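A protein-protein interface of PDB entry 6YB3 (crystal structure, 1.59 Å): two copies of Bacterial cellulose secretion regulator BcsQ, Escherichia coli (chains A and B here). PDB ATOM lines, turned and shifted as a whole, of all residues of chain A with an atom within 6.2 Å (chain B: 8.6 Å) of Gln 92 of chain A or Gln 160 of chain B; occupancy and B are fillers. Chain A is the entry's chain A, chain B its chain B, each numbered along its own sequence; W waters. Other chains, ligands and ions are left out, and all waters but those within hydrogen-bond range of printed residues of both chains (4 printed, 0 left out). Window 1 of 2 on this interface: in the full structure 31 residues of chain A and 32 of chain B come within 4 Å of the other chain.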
ATOM      1  N   PRO A  40     -21.590  13.060  10.072  1.00  0.00           N
ATOM      2  CA  PRO A  40     -22.645  12.032  10.047  1.00  0.00           C
ATOM      3  C   PRO A  40     -23.006  11.498  11.418  1.00  0.00           C
ATOM      4  O   PRO A  40     -24.083  10.907  11.562  1.00  0.00           O
ATOM      5  CB  PRO A  40     -22.043  10.929   9.162  1.00  0.00           C
ATOM      6  CG  PRO A  40     -21.017  11.639   8.328  1.00  0.00           C
ATOM      7  CD  PRO A  40     -20.457  12.726   9.197  1.00  0.00           C
ATOM      8  N   ASP A  41     -22.151  11.676  12.427  1.00  0.00           N
ATOM      9  CA  ASP A  41     -22.504  11.254  13.777  1.00  0.00           C
ATOM     10  C   ASP A  41     -23.560  12.147  14.424  1.00  0.00           C
ATOM     11  O   ASP A  41     -24.098  11.773  15.472  1.00  0.00           O
ATOM     12  CB  ASP A  41     -21.256  11.212  14.660  1.00  0.00           C
ATOM     13  CG  ASP A  41     -20.416  12.465  14.533  1.00  0.00           C
ATOM     14  OD1 ASP A  41     -19.572  12.526  13.620  1.00  0.00           O
ATOM     15  OD2 ASP A  41     -20.622  13.408  15.325  1.00  0.00           O
ATOM     16  N   LEU A  87     -28.756   8.854  10.725  1.00  0.00           N
ATOM     17  CA  LEU A  87     -28.647   7.820   9.703  1.00  0.00           C
ATOM     18  C   LEU A  87     -28.940   6.442  10.295  1.00  0.00           C
ATOM     19  O   LEU A  87     -28.648   6.171  11.461  1.00  0.00           O
ATOM     20  CB  LEU A  87     -27.248   7.818   9.082  1.00  0.00           C
ATOM     21  CG  LEU A  87     -26.737   9.069   8.366  1.00  0.00           C
ATOM     22  CD1 LEU A  87     -25.259   8.908   8.021  1.00  0.00           C
ATOM     23  CD2 LEU A  87     -27.551   9.338   7.117  1.00  0.00           C
ATOM     24  N   SER A  88     -29.509   5.563   9.474  1.00  0.00           N
ATOM     25  CA  SER A  88     -29.641   4.171   9.881  1.00  0.00           C
ATOM     26  C   SER A  88     -28.265   3.515   9.965  1.00  0.00           C
ATOM     27  O   SER A  88     -27.268   4.038   9.461  1.00  0.00           O
ATOM     28  CB  SER A  88     -30.512   3.400   8.898  1.00  0.00           C
ATOM     29  OG  SER A  88     -29.871   3.322   7.638  1.00  0.00           O
ATOM     30  N   ILE A  89     -28.217   2.346  10.608  1.00  0.00           N
ATOM     31  CA  ILE A  89     -26.961   1.602  10.659  1.00  0.00           C
ATOM     32  C   ILE A  89     -26.489   1.265   9.251  1.00  0.00           C
ATOM     33  O   ILE A  89     -25.295   1.350   8.940  1.00  0.00           O
ATOM     34  CB  ILE A  89     -27.113   0.339  11.529  1.00  0.00           C
ATOM     35  CG1 ILE A  89     -27.330   0.733  12.992  1.00  0.00           C
ATOM     36  CG2 ILE A  89     -25.893  -0.556  11.379  1.00  0.00           C
ATOM     37  CD1 ILE A  89     -27.266  -0.436  13.956  1.00  0.00           C
ATOM     38  N   GLU A  90     -27.424   0.903   8.369  1.00  0.00           N
ATOM     39  CA  GLU A  90     -27.066   0.594   6.990  1.00  0.00           C
ATOM     40  C   GLU A  90     -26.459   1.801   6.286  1.00  0.00           C
ATOM     41  O   GLU A  90     -25.473   1.667   5.549  1.00  0.00           O
ATOM     42  CB  GLU A  90     -28.294   0.083   6.235  1.00  0.00           C
ATOM     43  CG  GLU A  90     -28.003  -0.462   4.852  1.00  0.00           C
ATOM     44  CD  GLU A  90     -27.904   0.623   3.792  1.00  0.00           C
ATOM     45  OE1 GLU A  90     -27.270   0.377   2.740  1.00  0.00           O
ATOM     46  OE2 GLU A  90     -28.459   1.720   4.009  1.00  0.00           O
ATOM     47  N   GLU A  91     -27.041   2.986   6.477  1.00  0.00           N
ATOM     48  CA  GLU A  91     -26.467   4.185   5.878  1.00  0.00           C
ATOM     49  C   GLU A  91     -25.104   4.507   6.485  1.00  0.00           C
ATOM     50  O   GLU A  91     -24.174   4.895   5.764  1.00  0.00           O
ATOM     51  CB  GLU A  91     -27.431   5.361   6.043  1.00  0.00           C
ATOM     52  CG  GLU A  91     -28.681   5.234   5.191  1.00  0.00           C
ATOM     53  CD  GLU A  91     -29.731   6.277   5.531  1.00  0.00           C
ATOM     54  OE1 GLU A  91     -29.875   6.611   6.720  1.00  0.00           O
ATOM     55  OE2 GLU A  91     -30.419   6.754   4.605  1.00  0.00           O
ATOM     56  N   GLN A  92     -24.960   4.330   7.805  1.00  0.00           N
ATOM     57  CA  GLN A  92     -23.672   4.576   8.456  1.00  0.00           C
ATOM     58  C   GLN A  92     -22.560   3.714   7.861  1.00  0.00           C
ATOM     59  O   GLN A  92     -21.435   4.188   7.664  1.00  0.00           O
ATOM     60  CB  GLN A  92     -23.775   4.310   9.958  1.00  0.00           C
ATOM     61  CG  GLN A  92     -24.670   5.264  10.726  1.00  0.00           C
ATOM     62  CD  GLN A  92     -24.724   4.925  12.208  1.00  0.00           C
ATOM     63  OE1 GLN A  92     -23.697   4.635  12.828  1.00  0.00           O
ATOM     64  NE2 GLN A  92     -25.923   4.938  12.775  1.00  0.00           N
ATOM     65  N   GLU A  93     -22.835   2.438   7.607  1.00  0.00           N
ATOM     66  CA  GLU A  93     -21.791   1.535   7.146  1.00  0.00           C
ATOM     67  C   GLU A  93     -21.647   1.526   5.631  1.00  0.00           C
ATOM     68  O   GLU A  93     -20.843   0.755   5.100  1.00  0.00           O
ATOM     69  CB  GLU A  93     -22.054   0.120   7.663  1.00  0.00           C
ATOM     70  CG  GLU A  93     -22.090   0.034   9.184  1.00  0.00           C
ATOM     71  CD  GLU A  93     -20.845   0.616   9.836  1.00  0.00           C
ATOM     72  OE1 GLU A  93     -19.723   0.295   9.387  1.00  0.00           O
ATOM     73  OE2 GLU A  93     -20.991   1.402  10.799  1.00  0.00           O
ATOM     74  N   ASN A  94     -22.400   2.367   4.929  1.00  0.00           N
ATOM     75  CA  ASN A  94     -22.272   2.527   3.480  1.00  0.00           C
ATOM     76  C   ASN A  94     -22.149   4.007   3.131  1.00  0.00           C
ATOM     77  O   ASN A  94     -22.996   4.572   2.426  1.00  0.00           O
ATOM     78  CB  ASN A  94     -23.461   1.884   2.773  1.00  0.00           C
ATOM     79  CG  ASN A  94     -23.379   0.373   2.766  1.00  0.00           C
ATOM     80  OD1 ASN A  94     -22.736  -0.215   1.896  1.00  0.00           O
ATOM     81  ND2 ASN A  94     -24.019  -0.265   3.742  1.00  0.00           N
ATOM     82  N   PRO A  95     -21.086   4.672   3.603  1.00  0.00           N
ATOM     83  CA  PRO A  95     -20.971   6.121   3.365  1.00  0.00           C
ATOM     84  C   PRO A  95     -20.866   6.483   1.895  1.00  0.00           C
ATOM     85  O   PRO A  95     -21.279   7.582   1.504  1.00  0.00           O
ATOM     86  CB  PRO A  95     -19.696   6.500   4.131  1.00  0.00           C
ATOM     87  CG  PRO A  95     -18.894   5.233   4.178  1.00  0.00           C
ATOM     88  CD  PRO A  95     -19.890   4.121   4.276  1.00  0.00           C
ATOM     89  N   TRP A  98     -24.285   7.714   0.160  1.00  0.00           N
ATOM     90  CA  TRP A  98     -24.856   9.045   0.319  1.00  0.00           C
ATOM     91  C   TRP A  98     -23.842  10.179   0.288  1.00  0.00           C
ATOM     92  O   TRP A  98     -24.240  11.323   0.043  1.00  0.00           O
ATOM     93  CB  TRP A  98     -25.648   9.134   1.634  1.00  0.00           C
ATOM     94  CG  TRP A  98     -24.907   8.625   2.815  1.00  0.00           C
ATOM     95  CD1 TRP A  98     -25.019   7.388   3.374  1.00  0.00           C
ATOM     96  CD2 TRP A  98     -23.930   9.330   3.588  1.00  0.00           C
ATOM     97  NE1 TRP A  98     -24.176   7.276   4.446  1.00  0.00           N
ATOM     98  CE2 TRP A  98     -23.497   8.456   4.604  1.00  0.00           C
ATOM     99  CE3 TRP A  98     -23.387  10.618   3.529  1.00  0.00           C
ATOM    100  CZ2 TRP A  98     -22.538   8.819   5.541  1.00  0.00           C
ATOM    101  CZ3 TRP A  98     -22.439  10.981   4.462  1.00  0.00           C
ATOM    102  CH2 TRP A  98     -22.021  10.083   5.458  1.00  0.00           C
ATOM    103  N   GLN B   7     -10.562  -1.175  17.369  1.00  0.00           N
ATOM    104  CA  GLN B   7     -11.168  -0.069  16.637  1.00  0.00           C
ATOM    105  C   GLN B   7     -11.737   0.934  17.626  1.00  0.00           C
ATOM    106  O   GLN B   7     -12.505   0.566  18.518  1.00  0.00           O
ATOM    107  CB  GLN B   7     -12.266  -0.572  15.702  1.00  0.00           C
ATOM    108  CG  GLN B   7     -12.762   0.526  14.773  1.00  0.00           C
ATOM    109  CD  GLN B   7     -13.884   0.053  13.888  1.00  0.00           C
ATOM    110  OE1 GLN B   7     -14.777  -0.672  14.332  1.00  0.00           O
ATOM    111  NE2 GLN B   7     -13.832   0.434  12.612  1.00  0.00           N
ATOM    112  N   GLY B   8     -11.361   2.198  17.470  1.00  0.00           N
ATOM    113  CA  GLY B   8     -11.947   3.236  18.305  1.00  0.00           C
ATOM    114  C   GLY B   8     -13.414   3.460  17.978  1.00  0.00           C
ATOM    115  O   GLY B   8     -13.825   3.446  16.816  1.00  0.00           O
ATOM    116  N   VAL B   9     -14.217   3.670  19.030  1.00  0.00           N
ATOM    117  CA  VAL B   9     -15.609   4.079  18.843  1.00  0.00           C
ATOM    118  C   VAL B   9     -15.644   5.492  18.275  1.00  0.00           C
ATOM    119  O   VAL B   9     -16.582   5.865  17.559  1.00  0.00           O
ATOM    120  CB  VAL B   9     -16.374   3.938  20.175  1.00  0.00           C
ATOM    121  CG1 VAL B   9     -17.714   4.637  20.145  1.00  0.00           C
ATOM    122  CG2 VAL B   9     -16.564   2.444  20.501  1.00  0.00           C
ATOM    123  N   ARG B  10     -14.610   6.282  18.551  1.00  0.00           N
ATOM    124  CA  ARG B  10     -14.353   7.516  17.827  1.00  0.00           C
ATOM    125  C   ARG B  10     -12.846   7.673  17.716  1.00  0.00           C
ATOM    126  O   ARG B  10     -12.082   6.920  18.330  1.00  0.00           O
ATOM    127  CB  ARG B  10     -14.999   8.732  18.510  1.00  0.00           C
ATOM    128  CG  ARG B  10     -14.368   9.103  19.813  1.00  0.00           C
ATOM    129  CD  ARG B  10     -14.362  10.626  20.077  1.00  0.00           C
ATOM    130  NE  ARG B  10     -13.490  10.881  21.213  1.00  0.00           N
ATOM    131  CZ  ARG B  10     -13.911  10.957  22.473  1.00  0.00           C
ATOM    132  NH1 ARG B  10     -15.197  10.813  22.751  1.00  0.00           N
ATOM    133  NH2 ARG B  10     -13.045  11.161  23.463  1.00  0.00           N
ATOM    134  N   GLY B  11     -12.409   8.644  16.916  1.00  0.00           N
ATOM    135  CA  GLY B  11     -10.981   8.879  16.780  1.00  0.00           C
ATOM    136  C   GLY B  11     -10.353   9.355  18.080  1.00  0.00           C
ATOM    137  O   GLY B  11     -11.017   9.912  18.952  1.00  0.00           O
ATOM    138  N   ARG B 127     -11.374   4.454  12.397  1.00  0.00           N
ATOM    139  CA  ARG B 127     -12.760   4.850  12.637  1.00  0.00           C
ATOM    140  C   ARG B 127     -13.344   5.381  11.325  1.00  0.00           C
ATOM    141  O   ARG B 127     -13.540   6.578  11.122  1.00  0.00           O
ATOM    142  CB  ARG B 127     -12.818   5.884  13.758  1.00  0.00           C
ATOM    143  CG  ARG B 127     -14.199   6.494  14.065  1.00  0.00           C
ATOM    144  CD  ARG B 127     -15.125   5.495  14.724  1.00  0.00           C
ATOM    145  NE  ARG B 127     -15.932   4.758  13.758  1.00  0.00           N
ATOM    146  CZ  ARG B 127     -16.478   3.569  13.998  1.00  0.00           C
ATOM    147  NH1 ARG B 127     -16.290   2.974  15.164  1.00  0.00           N
ATOM    148  NH2 ARG B 127     -17.203   2.968  13.067  1.00  0.00           N
ATOM    149  N   ASP B 128     -13.563   4.458  10.392  1.00  0.00           N
ATOM    150  CA  ASP B 128     -14.344   4.742   9.204  1.00  0.00           C
ATOM    151  C   ASP B 128     -15.180   3.509   8.894  1.00  0.00           C
ATOM    152  O   ASP B 128     -15.187   2.530   9.649  1.00  0.00           O
ATOM    153  CB  ASP B 128     -13.474   5.193   8.007  1.00  0.00           C
ATOM    154  CG  ASP B 128     -12.497   4.122   7.512  1.00  0.00           C
ATOM    155  OD1 ASP B 128     -12.880   2.941   7.384  1.00  0.00           O
ATOM    156  OD2 ASP B 128     -11.340   4.481   7.190  1.00  0.00           O
ATOM    157  N   ALA B 129     -15.909   3.580   7.784  1.00  0.00           N
ATOM    158  CA  ALA B 129     -16.756   2.500   7.296  1.00  0.00           C
ATOM    159  C   ALA B 129     -16.380   2.127   5.870  1.00  0.00           C
ATOM    160  O   ALA B 129     -17.241   1.759   5.065  1.00  0.00           O
ATOM    161  CB  ALA B 129     -18.234   2.883   7.367  1.00  0.00           C
ATOM    162  N   SER B 130     -15.098   2.238   5.541  1.00  0.00           N
ATOM    163  CA  SER B 130     -14.675   1.974   4.180  1.00  0.00           C
ATOM    164  C   SER B 130     -14.762   0.481   3.876  1.00  0.00           C
ATOM    165  O   SER B 130     -14.850  -0.369   4.770  1.00  0.00           O
ATOM    166  CB  SER B 130     -13.250   2.473   3.952  1.00  0.00           C
ATOM    167  OG  SER B 130     -12.319   1.605   4.570  1.00  0.00           O
ATOM    168  N   HIS B 134     -14.175  -2.773   6.552  1.00  0.00           N
ATOM    169  CA  HIS B 134     -15.137  -3.854   6.745  1.00  0.00           C
ATOM    170  C   HIS B 134     -14.537  -5.197   6.367  1.00  0.00           C
ATOM    171  O   HIS B 134     -14.745  -6.199   7.062  1.00  0.00           O
ATOM    172  CB  HIS B 134     -16.393  -3.591   5.914  1.00  0.00           C
ATOM    173  CG  HIS B 134     -17.231  -2.468   6.434  1.00  0.00           C
ATOM    174  ND1 HIS B 134     -18.025  -1.693   5.616  1.00  0.00           N
ATOM    175  CD2 HIS B 134     -17.400  -1.990   7.689  1.00  0.00           C
ATOM    176  CE1 HIS B 134     -18.646  -0.784   6.345  1.00  0.00           C
ATOM    177  NE2 HIS B 134     -18.287  -0.943   7.607  1.00  0.00           N
ATOM    178  N   ALA B 145     -13.518  -2.603  21.116  1.00  0.00           N
ATOM    179  CA  ALA B 145     -14.007  -1.276  20.768  1.00  0.00           C
ATOM    180  C   ALA B 145     -13.512  -0.322  21.848  1.00  0.00           C
ATOM    181  O   ALA B 145     -13.905  -0.436  23.011  1.00  0.00           O
ATOM    182  CB  ALA B 145     -15.530  -1.275  20.666  1.00  0.00           C
ATOM    183  N   ILE B 146     -12.632   0.596  21.470  1.00  0.00           N
ATOM    184  CA  ILE B 146     -11.940   1.450  22.426  1.00  0.00           C
ATOM    185  C   ILE B 146     -12.783   2.698  22.679  1.00  0.00           C
ATOM    186  O   ILE B 146     -13.258   3.339  21.735  1.00  0.00           O
ATOM    187  CB  ILE B 146     -10.542   1.820  21.903  1.00  0.00           C
ATOM    188  CG1 ILE B 146      -9.791   0.577  21.419  1.00  0.00           C
ATOM    189  CG2 ILE B 146      -9.759   2.596  22.964  1.00  0.00           C
ATOM    190  CD1 ILE B 146      -9.655  -0.496  22.485  1.00  0.00           C
ATOM    191  N   VAL B 147     -12.988   3.040  23.960  1.00  0.00           N
ATOM    192  CA  VAL B 147     -13.758   4.218  24.349  1.00  0.00           C
ATOM    193  C   VAL B 147     -12.954   5.030  25.357  1.00  0.00           C
ATOM    194  O   VAL B 147     -11.986   4.550  25.954  1.00  0.00           O
ATOM    195  CB  VAL B 147     -15.141   3.877  24.965  1.00  0.00           C
ATOM    196  CG1 VAL B 147     -16.028   3.158  23.968  1.00  0.00           C
ATOM    197  CG2 VAL B 147     -14.970   3.037  26.259  1.00  0.00           C
ATOM    198  N   ASN B 152     -19.545  12.094  24.742  1.00  0.00           N
ATOM    199  CA  ASN B 152     -19.475  11.748  23.326  1.00  0.00           C
ATOM    200  C   ASN B 152     -19.506  10.229  23.124  1.00  0.00           C
ATOM    201  O   ASN B 152     -20.347   9.714  22.383  1.00  0.00           O
ATOM    202  CB  ASN B 152     -18.221  12.410  22.733  1.00  0.00           C
ATOM    203  CG  ASN B 152     -17.914  11.998  21.296  1.00  0.00           C
ATOM    204  OD1 ASN B 152     -17.939  10.821  20.940  1.00  0.00           O
ATOM    205  ND2 ASN B 152     -17.541  12.980  20.477  1.00  0.00           N
ATOM    206  N   CYS B 153     -18.640   9.482  23.820  1.00  0.00           N
ATOM    207  CA  CYS B 153     -18.677   8.034  23.648  1.00  0.00           C
ATOM    208  C   CYS B 153     -19.990   7.456  24.158  1.00  0.00           C
ATOM    209  O   CYS B 153     -20.529   6.511  23.568  1.00  0.00           O
ATOM    210  CB  CYS B 153     -17.479   7.374  24.346  1.00  0.00           C
ATOM    211  SG  CYS B 153     -15.937   7.493  23.391  1.00  0.00           S
ATOM    212  N   HIS B 154     -20.518   8.008  25.255  1.00  0.00           N
ATOM    213  CA  HIS B 154     -21.816   7.573  25.765  1.00  0.00           C
ATOM    214  C   HIS B 154     -22.887   7.641  24.685  1.00  0.00           C
ATOM    215  O   HIS B 154     -23.609   6.667  24.439  1.00  0.00           O
ATOM    216  CB  HIS B 154     -22.228   8.427  26.961  1.00  0.00           C
ATOM    217  CG  HIS B 154     -23.470   7.943  27.642  1.00  0.00           C
ATOM    218  ND1 HIS B 154     -23.486   6.826  28.454  1.00  0.00           N
ATOM    219  CD2 HIS B 154     -24.739   8.412  27.620  1.00  0.00           C
ATOM    220  CE1 HIS B 154     -24.712   6.634  28.909  1.00  0.00           C
ATOM    221  NE2 HIS B 154     -25.491   7.586  28.421  1.00  0.00           N
ATOM    222  N   ILE B 155     -23.007   8.795  24.032  1.00  0.00           N
ATOM    223  CA  ILE B 155     -23.990   8.933  22.960  1.00  0.00           C
ATOM    224  C   ILE B 155     -23.724   7.907  21.865  1.00  0.00           C
ATOM    225  O   ILE B 155     -24.644   7.248  21.362  1.00  0.00           O
ATOM    226  CB  ILE B 155     -23.960  10.360  22.388  1.00  0.00           C
ATOM    227  CG1 ILE B 155     -24.407  11.385  23.434  1.00  0.00           C
ATOM    228  CG2 ILE B 155     -24.835  10.445  21.130  1.00  0.00           C
ATOM    229  CD1 ILE B 155     -23.823  12.774  23.201  1.00  0.00           C
ATOM    230  N   ARG B 156     -22.457   7.776  21.466  1.00  0.00           N
ATOM    231  CA  ARG B 156     -22.126   6.929  20.325  1.00  0.00           C
ATOM    232  C   ARG B 156     -22.553   5.493  20.576  1.00  0.00           C
ATOM    233  O   ARG B 156     -23.019   4.811  19.660  1.00  0.00           O
ATOM    234  CB  ARG B 156     -20.626   7.008  20.021  1.00  0.00           C
ATOM    235  CG  ARG B 156     -20.192   8.310  19.327  1.00  0.00           C
ATOM    236  CD  ARG B 156     -18.679   8.333  19.118  1.00  0.00           C
ATOM    237  NE  ARG B 156     -18.244   9.489  18.339  1.00  0.00           N
ATOM    238  CZ  ARG B 156     -18.167   9.498  17.009  1.00  0.00           C
ATOM    239  NH1 ARG B 156     -18.486   8.409  16.317  1.00  0.00           N
ATOM    240  NH2 ARG B 156     -17.767  10.592  16.363  1.00  0.00           N
ATOM    241  N   LEU B 157     -22.452   5.037  21.827  1.00  0.00           N
ATOM    242  CA  LEU B 157     -22.825   3.667  22.158  1.00  0.00           C
ATOM    243  C   LEU B 157     -24.328   3.416  22.053  1.00  0.00           C
ATOM    244  O   LEU B 157     -24.741   2.251  22.069  1.00  0.00           O
ATOM    245  CB  LEU B 157     -22.324   3.318  23.561  1.00  0.00           C
ATOM    246  CG  LEU B 157     -20.808   3.164  23.739  1.00  0.00           C
ATOM    247  CD1 LEU B 157     -20.470   2.908  25.217  1.00  0.00           C
ATOM    248  CD2 LEU B 157     -20.257   2.033  22.878  1.00  0.00           C
ATOM    249  N   HIS B 158     -25.153   4.460  21.933  1.00  0.00           N
ATOM    250  CA  HIS B 158     -26.587   4.290  21.723  1.00  0.00           C
ATOM    251  C   HIS B 158     -27.004   4.448  20.270  1.00  0.00           C
ATOM    252  O   HIS B 158     -28.194   4.307  19.966  1.00  0.00           O
ATOM    253  CB  HIS B 158     -27.379   5.285  22.578  1.00  0.00           C
ATOM    254  CG  HIS B 158     -27.138   5.138  24.047  1.00  0.00           C
ATOM    255  ND1 HIS B 158     -26.023   5.652  24.672  1.00  0.00           N
ATOM    256  CD2 HIS B 158     -27.871   4.539  25.017  1.00  0.00           C
ATOM    257  CE1 HIS B 158     -26.078   5.378  25.964  1.00  0.00           C
ATOM    258  NE2 HIS B 158     -27.195   4.710  26.201  1.00  0.00           N
ATOM    259  N   GLN B 159     -26.070   4.738  19.363  1.00  0.00           N
ATOM    260  CA  GLN B 159     -26.474   5.029  17.988  1.00  0.00           C
ATOM    261  C   GLN B 159     -25.579   4.446  16.908  1.00  0.00           C
ATOM    262  O   GLN B 159     -26.013   4.410  15.754  1.00  0.00           O
ATOM    263  CB  GLN B 159     -26.570   6.542  17.764  1.00  0.00           C
ATOM    264  CG  GLN B 159     -25.237   7.260  17.777  1.00  0.00           C
ATOM    265  CD  GLN B 159     -25.371   8.737  17.449  1.00  0.00           C
ATOM    266  OE1 GLN B 159     -26.456   9.316  17.561  1.00  0.00           O
ATOM    267  NE2 GLN B 159     -24.268   9.351  17.036  1.00  0.00           N
ATOM    268  N   GLN B 160     -24.358   3.997  17.191  1.00  0.00           N
ATOM    269  CA  GLN B 160     -23.536   3.434  16.133  1.00  0.00           C
ATOM    270  C   GLN B 160     -23.296   1.958  16.412  1.00  0.00           C
ATOM    271  O   GLN B 160     -23.164   1.544  17.567  1.00  0.00           O
ATOM    272  CB  GLN B 160     -22.210   4.206  15.949  1.00  0.00           C
ATOM    273  CG  GLN B 160     -21.100   3.874  16.891  1.00  0.00           C
ATOM    274  CD  GLN B 160     -19.896   4.793  16.713  1.00  0.00           C
ATOM    275  OE1 GLN B 160     -20.035   6.014  16.681  1.00  0.00           O
ATOM    276  NE2 GLN B 160     -18.705   4.204  16.620  1.00  0.00           N
ATOM    277  N   ALA B 161     -23.321   1.170  15.346  1.00  0.00           N
ATOM    278  CA  ALA B 161     -23.138  -0.265  15.456  1.00  0.00           C
ATOM    279  C   ALA B 161     -21.681  -0.594  15.732  1.00  0.00           C
ATOM    280  O   ALA B 161     -20.768   0.080  15.243  1.00  0.00           O
ATOM    281  CB  ALA B 161     -23.593  -0.961  14.173  1.00  0.00           C
ATOM    282  N   LEU B 162     -21.470  -1.625  16.523  1.00  0.00           N
ATOM    283  CA  LEU B 162     -20.152  -2.177  16.721  1.00  0.00           C
ATOM    284  C   LEU B 162     -20.083  -3.546  16.069  1.00  0.00           C
ATOM    285  O   LEU B 162     -21.119  -4.170  15.809  1.00  0.00           O
ATOM    286  CB  LEU B 162     -19.826  -2.300  18.215  1.00  0.00           C
ATOM    287  CG  LEU B 162     -19.793  -0.986  18.992  1.00  0.00           C
ATOM    288  CD1 LEU B 162     -19.218  -1.239  20.366  1.00  0.00           C
ATOM    289  CD2 LEU B 162     -18.993   0.072  18.241  1.00  0.00           C
ATOM    290  N   PRO B 163     -18.885  -4.034  15.760  1.00  0.00           N
ATOM    291  CA  PRO B 163     -18.765  -5.409  15.270  1.00  0.00           C
ATOM    292  C   PRO B 163     -19.432  -6.358  16.253  1.00  0.00           C
ATOM    293  O   PRO B 163     -19.304  -6.202  17.467  1.00  0.00           O
ATOM    294  CB  PRO B 163     -17.251  -5.626  15.201  1.00  0.00           C
ATOM    295  CG  PRO B 163     -16.683  -4.267  15.046  1.00  0.00           C
ATOM    296  CD  PRO B 163     -17.581  -3.352  15.823  1.00  0.00           C
HETATM  297  O   HOH W   1     -26.630  12.129  17.771  1.00  0.00           O
HETATM  298  O   HOH W   2     -22.999   2.006  12.624  1.00  0.00           O
HETATM  299  O   HOH W   3     -16.733   0.148  10.646  1.00  0.00           O
HETATM  300  O   HOH W   4     -24.123   7.158  14.418  1.00  0.00           O
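The side-chain amide nitrogen of Gln 159 of chain B lies within hydrogen-bond range of the backbone carbonyl oxygen of Asp 41 of chain A, 2.9 Å away.
NH2 of Arg 156 of chain B is in salt-bridge range of OD1 of Asp 41 of chain A (3.8 Å).
The side-chain amide nitrogen (NE2) of Gln 92 of chain A is in hydrogen-bond range of the backbone carbonyl oxygen (O) of Gln 159 of chain B (3.0 Å).
OE1 of Glu 93 of chain A is in hydrogen-bond range of NE2 of His 134 of chain B (2.6 Å).
O of Leu 87 of chain A is in hydrogen-bond range of NE2 of Gln 92 of chain A (3.3 Å).
The guanidinium group of Arg 127 of chain B sits close to the side-chain amide nitrogen of Gln 160 of chain B (3.1 Å).
The backbone carbonyl oxygen (O) of Val 9 of chain B is in hydrogen-bond range of the side-chain amide nitrogen (NE2) of Gln 160 of chain B (2.9 Å).
The backbone carbonyl oxygen of Val 9 of chain B sits at hydrogen-bond distance from the guanidinium group of Arg 156 of chain B (3.4 Å).
The side-chain amide oxygen (OD1) of Asn 152 of chain B sits at hydrogen-bond distance from the guanidinium group (NE) of Arg 156 of chain B, 2.9 Å away.
NH1 of Arg 156 of chain B lies within hydrogen-bond range of OE1 of Gln 160 of chain B (2.9 Å).
Among the printed residues, merely in contact across the chains: Ile 89 of chain A with Ala 161 of chain B (3.6 Å), Gln 92 of chain A with Ala 129 of chain B (3.5 Å), Gln 92 of chain A with Gln 160 of chain B (3.5 Å), Glu 93 of chain A with Ala 129 of chain B (3.6 Å) and Pro 95 of chain A with Ala 129 of chain B (3.6 Å).
Printed residues of chain B within 4 Å of Gln 92 of chain A: Ala 129 (3.5 Å), Gln 159 (3.0 Å) and Gln 160 (3.5 Å).
Of chain A, only Gln 92 (3.5 Å) comes within 4 Å of Gln 160 of chain B.
Of the printed residues of chain A, Ala 129 of chain B touches Gln 92, Glu 93 and Pro 95.
Of the printed residues of chain A, Gln 159 of chain B touches Asp 41 and Gln 92.
The nearest printed residue of chain A that does not touch His 134 of chain B is Asn 94 of chain A (5.1 Å).
Of the 12 printed residues of chain A, 5 touch a printed residue of chain B.
Printed residues of chain A that touch a printed residue of chain B: Asp 41, Ile 89, Gln 92, Glu 93 and Pro 95.
Hydrophobic or aromatic side chains of chain A within 4 Å of the printed part of chain B: Ile 89 and Pro 95.
Hydrophobic or aromatic side chains of chain B that line the printed part of chain A: Ala 129, His 134 and Ala 161.
Among the printed residues, 9 pairs touch across the chains.
No position is printed for both chains.
Of the 9 pairs that touch across the chains among the printed residues, none has its exchanged pair printed and touching as well.
Water W2 lies within hydrogen-bond range of OE1 of Gln 92 of chain A (2.7 Å), OE2 of Glu 93 of chain A (2.8 Å) and N of Ala 161 of chain B (2.9 Å).
Water W1 lies within hydrogen-bond range of the side-chain amide oxygen of Gln 159 of chain B (2.8 Å) and the backbone carbonyl oxygen of Asp 41 of chain A (3.4 Å).
Water W3 bridges the backbone carbonyl oxygen of Asp 128 of chain B and the side-chain carboxylate of Glu 93 of chain A.
Water W4 bridges OE1 of Gln 92 of chain A (3.0 Å) and NE2 of Gln 159 of chain B (3.4 Å).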
